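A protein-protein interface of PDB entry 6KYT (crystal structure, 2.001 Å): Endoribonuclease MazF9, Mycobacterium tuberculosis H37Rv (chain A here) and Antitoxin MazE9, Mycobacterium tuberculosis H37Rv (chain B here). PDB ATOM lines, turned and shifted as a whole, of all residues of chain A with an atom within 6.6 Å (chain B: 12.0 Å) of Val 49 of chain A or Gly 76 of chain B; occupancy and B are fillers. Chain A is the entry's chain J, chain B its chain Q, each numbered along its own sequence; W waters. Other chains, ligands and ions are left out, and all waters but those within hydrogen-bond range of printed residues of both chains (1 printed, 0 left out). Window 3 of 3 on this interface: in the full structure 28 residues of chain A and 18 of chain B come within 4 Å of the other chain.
Water W1 lies within hydrogen-bond range of O of Ser 89 of chain A (2.8 Å) and O of Thr 72 of chain B (3.1 Å).
The backbone NH of Ala 91 of chain A sits at hydrogen-bond distance from the side-chain carboxylate of Asp 75 of chain B (2.9 Å).
Val 49 of chain A touches Gly 76 of chain B.
Ser 89 of chain A touches Asp 75 of chain B.
Thr 72 of chain B touches Ile 90 of chain A (CB to CG2, 3.6 Å).
Asp 75 of chain B touches Ile 90 of chain A.
No residue of chain B comes within 4 Å of Ala 38 of chain A.
No residue of chain B comes within 4 Å of Ala 42 of chain A.
No residue of chain B comes within 4 Å of Leu 45 of chain A.
No residue of chain B comes within 4 Å of Gly 48 of chain A.
Val 49 of chain A touches one residue of chain B.
No residue of chain B comes within 4 Å of Ile 50 of chain A.
No residue of chain B comes within 4 Å of Thr 51 of chain A.
Of chain B, only Asp 75 comes within 4 Å of Ala 91 of chain A.
No residue of chain B comes within 4 Å of Thr 92 of chain A.
Of the printed residues of chain A, Thr 72 of chain B touches Ile 90 (3.6 Å).
Of the printed residues of chain A, Asp 75 of chain B touches Ser 89, Ile 90 and Ala 91.
Gly 76 of chain B touches just one residue of chain A: Val 49 (3.6 Å).
The nearest residue of chain B that does not touch Val 49 of chain A is Asp 75 of chain B (4.1 Å).
The nearest residue of chain A that does not touch Gly 76 of chain B is Ala 91 of chain A (5.3 Å).
The nearest printed residue of chain A that does not touch Asp 75 of chain B is Val 49 of chain A (4.1 Å).
The backbone carbonyl oxygen of Ile 90 of chain A sits at hydrogen-bond distance from the backbone NH of Ile 50 of chain A, 2.9 Å away.
The side-chain hydroxyl (OG1) of Thr 51 of chain A is in hydrogen-bond range of the side-chain hydroxyl (OG) of Ser 89 of chain A (3.0 Å).
The side-chain hydroxyl (OG1) of Thr 72 of chain B sits at hydrogen-bond distance from the backbone carbonyl oxygen (O) of Trp 69 of chain B, 2.8 Å away.
Among the printed residues, no Asp or Glu carboxylate lies within 4 Å of a Lys or Arg side-chain nitrogen of the other chain.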
ATOM      1  N   SER A  34     -19.392  20.362  29.562  1.00  0.00           N
ATOM      2  CA  SER A  34     -20.426  19.931  30.491  1.00  0.00           C
ATOM      3  C   SER A  34     -20.525  20.917  31.649  1.00  0.00           C
ATOM      4  O   SER A  34     -19.562  21.610  31.986  1.00  0.00           O
ATOM      5  CB  SER A  34     -20.130  18.526  31.017  1.00  0.00           C
ATOM      6  OG  SER A  34     -18.750  18.364  31.282  1.00  0.00           O
ATOM      7  N   ALA A  38     -22.546  18.705  36.937  1.00  0.00           N
ATOM      8  CA  ALA A  38     -22.226  17.389  36.398  1.00  0.00           C
ATOM      9  C   ALA A  38     -20.742  17.079  36.536  1.00  0.00           C
ATOM     10  O   ALA A  38     -20.362  15.926  36.768  1.00  0.00           O
ATOM     11  CB  ALA A  38     -22.659  17.303  34.935  1.00  0.00           C
ATOM     12  N   ASN A  39     -19.881  18.091  36.396  1.00  0.00           N
ATOM     13  CA  ASN A  39     -18.449  17.849  36.555  1.00  0.00           C
ATOM     14  C   ASN A  39     -18.108  17.509  38.002  1.00  0.00           C
ATOM     15  O   ASN A  39     -17.392  16.533  38.270  1.00  0.00           O
ATOM     16  CB  ASN A  39     -17.658  19.064  36.068  1.00  0.00           C
ATOM     17  CG  ASN A  39     -17.852  19.326  34.584  1.00  0.00           C
ATOM     18  OD1 ASN A  39     -18.011  18.393  33.796  1.00  0.00           O
ATOM     19  ND2 ASN A  39     -17.848  20.597  34.197  1.00  0.00           N
ATOM     20  N   ALA A  42     -18.985  14.202  38.647  1.00  0.00           N
ATOM     21  CA  ALA A  42     -18.193  13.274  37.847  1.00  0.00           C
ATOM     22  C   ALA A  42     -16.854  12.960  38.500  1.00  0.00           C
ATOM     23  O   ALA A  42     -16.378  11.822  38.420  1.00  0.00           O
ATOM     24  CB  ALA A  42     -17.981  13.845  36.444  1.00  0.00           C
ATOM     25  N   LEU A  45     -17.783  10.190  40.954  1.00  0.00           N
ATOM     26  CA  LEU A  45     -18.224   8.912  40.385  1.00  0.00           C
ATOM     27  C   LEU A  45     -17.034   8.091  39.883  1.00  0.00           C
ATOM     28  O   LEU A  45     -17.046   6.862  39.932  1.00  0.00           O
ATOM     29  CB  LEU A  45     -19.221   9.128  39.244  1.00  0.00           C
ATOM     30  N   GLY A  48     -17.437   7.999  35.942  1.00  0.00           N
ATOM     31  CA  GLY A  48     -17.961   9.287  35.527  1.00  0.00           C
ATOM     32  C   GLY A  48     -17.265   9.845  34.300  1.00  0.00           C
ATOM     33  O   GLY A  48     -16.102   9.536  34.045  1.00  0.00           O
ATOM     34  N   VAL A  49     -17.979  10.675  33.538  1.00  0.00           N
ATOM     35  CA  VAL A  49     -17.454  11.253  32.310  1.00  0.00           C
ATOM     36  C   VAL A  49     -17.681  12.759  32.313  1.00  0.00           C
ATOM     37  O   VAL A  49     -18.584  13.280  32.972  1.00  0.00           O
ATOM     38  CB  VAL A  49     -18.087  10.624  31.048  1.00  0.00           C
ATOM     39  CG1 VAL A  49     -17.713   9.155  30.936  1.00  0.00           C
ATOM     40  CG2 VAL A  49     -19.599  10.797  31.069  1.00  0.00           C
ATOM     41  N   ILE A  50     -16.831  13.454  31.562  1.00  0.00           N
ATOM     42  CA  ILE A  50     -16.944  14.884  31.309  1.00  0.00           C
ATOM     43  C   ILE A  50     -17.006  15.092  29.805  1.00  0.00           C
ATOM     44  O   ILE A  50     -16.256  14.461  29.049  1.00  0.00           O
ATOM     45  CB  ILE A  50     -15.763  15.669  31.913  1.00  0.00           C
ATOM     46  CG1 ILE A  50     -15.809  15.573  33.430  1.00  0.00           C
ATOM     47  CG2 ILE A  50     -15.780  17.123  31.463  1.00  0.00           C
ATOM     48  CD1 ILE A  50     -14.810  14.627  33.957  1.00  0.00           C
ATOM     49  N   THR A  51     -17.902  15.970  29.374  1.00  0.00           N
ATOM     50  CA  THR A  51     -18.054  16.278  27.962  1.00  0.00           C
ATOM     51  C   THR A  51     -17.105  17.407  27.581  1.00  0.00           C
ATOM     52  O   THR A  51     -17.112  18.472  28.208  1.00  0.00           O
ATOM     53  CB  THR A  51     -19.499  16.658  27.651  1.00  0.00           C
ATOM     54  OG1 THR A  51     -20.380  15.748  28.323  1.00  0.00           O
ATOM     55  CG2 THR A  51     -19.750  16.573  26.164  1.00  0.00           C
ATOM     56  N   SER A  89     -17.755  12.690  25.267  1.00  0.00           N
ATOM     57  CA  SER A  89     -17.763  12.489  26.711  1.00  0.00           C
ATOM     58  C   SER A  89     -16.705  11.449  27.057  1.00  0.00           C
ATOM     59  O   SER A  89     -16.764  10.315  26.571  1.00  0.00           O
ATOM     60  CB  SER A  89     -19.142  12.051  27.200  1.00  0.00           C
ATOM     61  OG  SER A  89     -20.107  13.057  26.955  1.00  0.00           O
ATOM     62  N   ILE A  90     -15.738  11.836  27.892  1.00  0.00           N
ATOM     63  CA  ILE A  90     -14.580  11.002  28.179  1.00  0.00           C
ATOM     64  C   ILE A  90     -14.462  10.786  29.682  1.00  0.00           C
ATOM     65  O   ILE A  90     -14.939  11.585  30.490  1.00  0.00           O
ATOM     66  CB  ILE A  90     -13.275  11.609  27.622  1.00  0.00           C
ATOM     67  CG1 ILE A  90     -12.962  12.938  28.313  1.00  0.00           C
ATOM     68  CG2 ILE A  90     -13.386  11.816  26.123  1.00  0.00           C
ATOM     69  CD1 ILE A  90     -11.710  13.611  27.790  1.00  0.00           C
ATOM     70  N   ALA A  91     -13.804   9.688  30.049  1.00  0.00           N
ATOM     71  CA  ALA A  91     -13.678   9.318  31.453  1.00  0.00           C
ATOM     72  C   ALA A  91     -12.903  10.377  32.229  1.00  0.00           C
ATOM     73  O   ALA A  91     -11.906  10.921  31.745  1.00  0.00           O
ATOM     74  CB  ALA A  91     -12.991   7.959  31.578  1.00  0.00           C
ATOM     75  N   THR A  92     -13.371  10.655  33.452  1.00  0.00           N
ATOM     76  CA  THR A  92     -12.800  11.725  34.268  1.00  0.00           C
ATOM     77  C   THR A  92     -11.298  11.561  34.449  1.00  0.00           C
ATOM     78  O   THR A  92     -10.553  12.550  34.457  1.00  0.00           O
ATOM     79  CB  THR A  92     -13.491  11.760  35.634  1.00  0.00           C
ATOM     80  OG1 THR A  92     -14.904  11.911  35.455  1.00  0.00           O
ATOM     81  CG2 THR A  92     -12.963  12.912  36.481  1.00  0.00           C
ATOM     82  N   GLU A  93     -10.836  10.316  34.586  1.00  0.00           N
ATOM     83  CA  GLU A  93      -9.425  10.054  34.839  1.00  0.00           C
ATOM     84  C   GLU A  93      -8.526  10.575  33.726  1.00  0.00           C
ATOM     85  O   GLU A  93      -7.347  10.840  33.977  1.00  0.00           O
ATOM     86  CB  GLU A  93      -9.198   8.552  35.036  1.00  0.00           C
ATOM     87  CG  GLU A  93     -10.302   7.847  35.834  1.00  0.00           C
ATOM     88  CD  GLU A  93     -11.527   7.499  34.974  1.00  0.00           C
ATOM     89  OE1 GLU A  93     -11.367   6.734  33.987  1.00  0.00           O
ATOM     90  OE2 GLU A  93     -12.636   8.014  35.275  1.00  0.00           O
ATOM     91  N   TRP B  69      -8.335  10.215  19.567  1.00  0.00           N
ATOM     92  CA  TRP B  69      -9.615  10.466  20.222  1.00  0.00           C
ATOM     93  C   TRP B  69     -10.536   9.257  20.146  1.00  0.00           C
ATOM     94  O   TRP B  69     -11.356   9.046  21.051  1.00  0.00           O
ATOM     95  CB  TRP B  69     -10.288  11.693  19.609  1.00  0.00           C
ATOM     96  CG  TRP B  69      -9.733  12.965  20.145  1.00  0.00           C
ATOM     97  CD1 TRP B  69      -8.797  13.766  19.560  1.00  0.00           C
ATOM     98  CD2 TRP B  69     -10.058  13.574  21.400  1.00  0.00           C
ATOM     99  NE1 TRP B  69      -8.529  14.845  20.368  1.00  0.00           N
ATOM    100  CE2 TRP B  69      -9.289  14.750  21.504  1.00  0.00           C
ATOM    101  CE3 TRP B  69     -10.928  13.241  22.441  1.00  0.00           C
ATOM    102  CZ2 TRP B  69      -9.366  15.595  22.609  1.00  0.00           C
ATOM    103  CZ3 TRP B  69     -11.003  14.081  23.537  1.00  0.00           C
ATOM    104  CH2 TRP B  69     -10.228  15.244  23.612  1.00  0.00           C
ATOM    105  N   GLU B  70     -10.402   8.442  19.094  1.00  0.00           N
ATOM    106  CA  GLU B  70     -11.222   7.238  18.984  1.00  0.00           C
ATOM    107  C   GLU B  70     -11.116   6.378  20.235  1.00  0.00           C
ATOM    108  O   GLU B  70     -12.101   5.748  20.636  1.00  0.00           O
ATOM    109  CB  GLU B  70     -10.820   6.439  17.742  1.00  0.00           C
ATOM    110  CG  GLU B  70     -11.569   5.122  17.551  1.00  0.00           C
ATOM    111  CD  GLU B  70     -11.435   4.579  16.137  1.00  0.00           C
ATOM    112  OE1 GLU B  70     -12.465   4.193  15.542  1.00  0.00           O
ATOM    113  OE2 GLU B  70     -10.301   4.552  15.611  1.00  0.00           O
ATOM    114  N   GLN B  71      -9.950   6.378  20.891  1.00  0.00           N
ATOM    115  CA  GLN B  71      -9.737   5.567  22.085  1.00  0.00           C
ATOM    116  C   GLN B  71     -10.755   5.840  23.188  1.00  0.00           C
ATOM    117  O   GLN B  71     -10.857   5.035  24.121  1.00  0.00           O
ATOM    118  CB  GLN B  71      -8.324   5.796  22.628  1.00  0.00           C
ATOM    119  CG  GLN B  71      -7.779   4.631  23.435  1.00  0.00           C
ATOM    120  CD  GLN B  71      -7.610   3.388  22.591  1.00  0.00           C
ATOM    121  OE1 GLN B  71      -8.037   2.299  22.973  1.00  0.00           O
ATOM    122  NE2 GLN B  71      -6.983   3.546  21.431  1.00  0.00           N
ATOM    123  N   THR B  72     -11.510   6.937  23.110  1.00  0.00           N
ATOM    124  CA  THR B  72     -12.478   7.272  24.147  1.00  0.00           C
ATOM    125  C   THR B  72     -13.903   6.853  23.809  1.00  0.00           C
ATOM    126  O   THR B  72     -14.806   7.100  24.615  1.00  0.00           O
ATOM    127  CB  THR B  72     -12.457   8.778  24.423  1.00  0.00           C
ATOM    128  OG1 THR B  72     -13.006   9.479  23.299  1.00  0.00           O
ATOM    129  CG2 THR B  72     -11.037   9.253  24.663  1.00  0.00           C
ATOM    130  N   VAL B  73     -14.127   6.218  22.655  1.00  0.00           N
ATOM    131  CA  VAL B  73     -15.488   5.983  22.174  1.00  0.00           C
ATOM    132  C   VAL B  73     -16.320   5.157  23.150  1.00  0.00           C
ATOM    133  O   VAL B  73     -17.552   5.265  23.155  1.00  0.00           O
ATOM    134  CB  VAL B  73     -15.451   5.319  20.774  1.00  0.00           C
ATOM    135  CG1 VAL B  73     -14.889   3.910  20.850  1.00  0.00           C
ATOM    136  CG2 VAL B  73     -16.837   5.315  20.143  1.00  0.00           C
ATOM    137  N   GLY B  74     -15.683   4.356  24.001  1.00  0.00           N
ATOM    138  CA  GLY B  74     -16.425   3.517  24.923  1.00  0.00           C
ATOM    139  C   GLY B  74     -16.363   3.952  26.372  1.00  0.00           C
ATOM    140  O   GLY B  74     -16.634   3.154  27.275  1.00  0.00           O
ATOM    141  N   ASP B  75     -16.014   5.212  26.611  1.00  0.00           N
ATOM    142  CA  ASP B  75     -15.929   5.721  27.972  1.00  0.00           C
ATOM    143  C   ASP B  75     -17.319   5.881  28.577  1.00  0.00           C
ATOM    144  O   ASP B  75     -18.267   6.287  27.899  1.00  0.00           O
ATOM    145  CB  ASP B  75     -15.190   7.058  27.992  1.00  0.00           C
ATOM    146  CG  ASP B  75     -13.695   6.899  27.803  1.00  0.00           C
ATOM    147  OD1 ASP B  75     -13.253   5.782  27.461  1.00  0.00           O
ATOM    148  OD2 ASP B  75     -12.962   7.891  27.997  1.00  0.00           O
ATOM    149  N   GLY B  76     -17.435   5.552  29.862  1.00  0.00           N
ATOM    150  CA  GLY B  76     -18.691   5.663  30.571  1.00  0.00           C
ATOM    151  C   GLY B  76     -19.724   4.611  30.238  1.00  0.00           C
ATOM    152  O   GLY B  76     -20.808   4.626  30.831  1.00  0.00           O
ATOM    153  N   VAL B  77     -19.432   3.705  29.309  1.00  0.00           N
ATOM    154  CA  VAL B  77     -20.371   2.655  28.933  1.00  0.00           C
ATOM    155  C   VAL B  77     -19.641   1.323  28.806  1.00  0.00           C
ATOM    156  O   VAL B  77     -20.128   0.290  29.267  1.00  0.00           O
ATOM    157  CB  VAL B  77     -21.105   3.000  27.623  1.00  0.00           C
ATOM    158  CG1 VAL B  77     -22.064   4.165  27.834  1.00  0.00           C
ATOM    159  CG2 VAL B  77     -20.104   3.321  26.525  1.00  0.00           C
HETATM  160  O   HOH W   1     -16.929   9.217  24.048  1.00  0.00           O
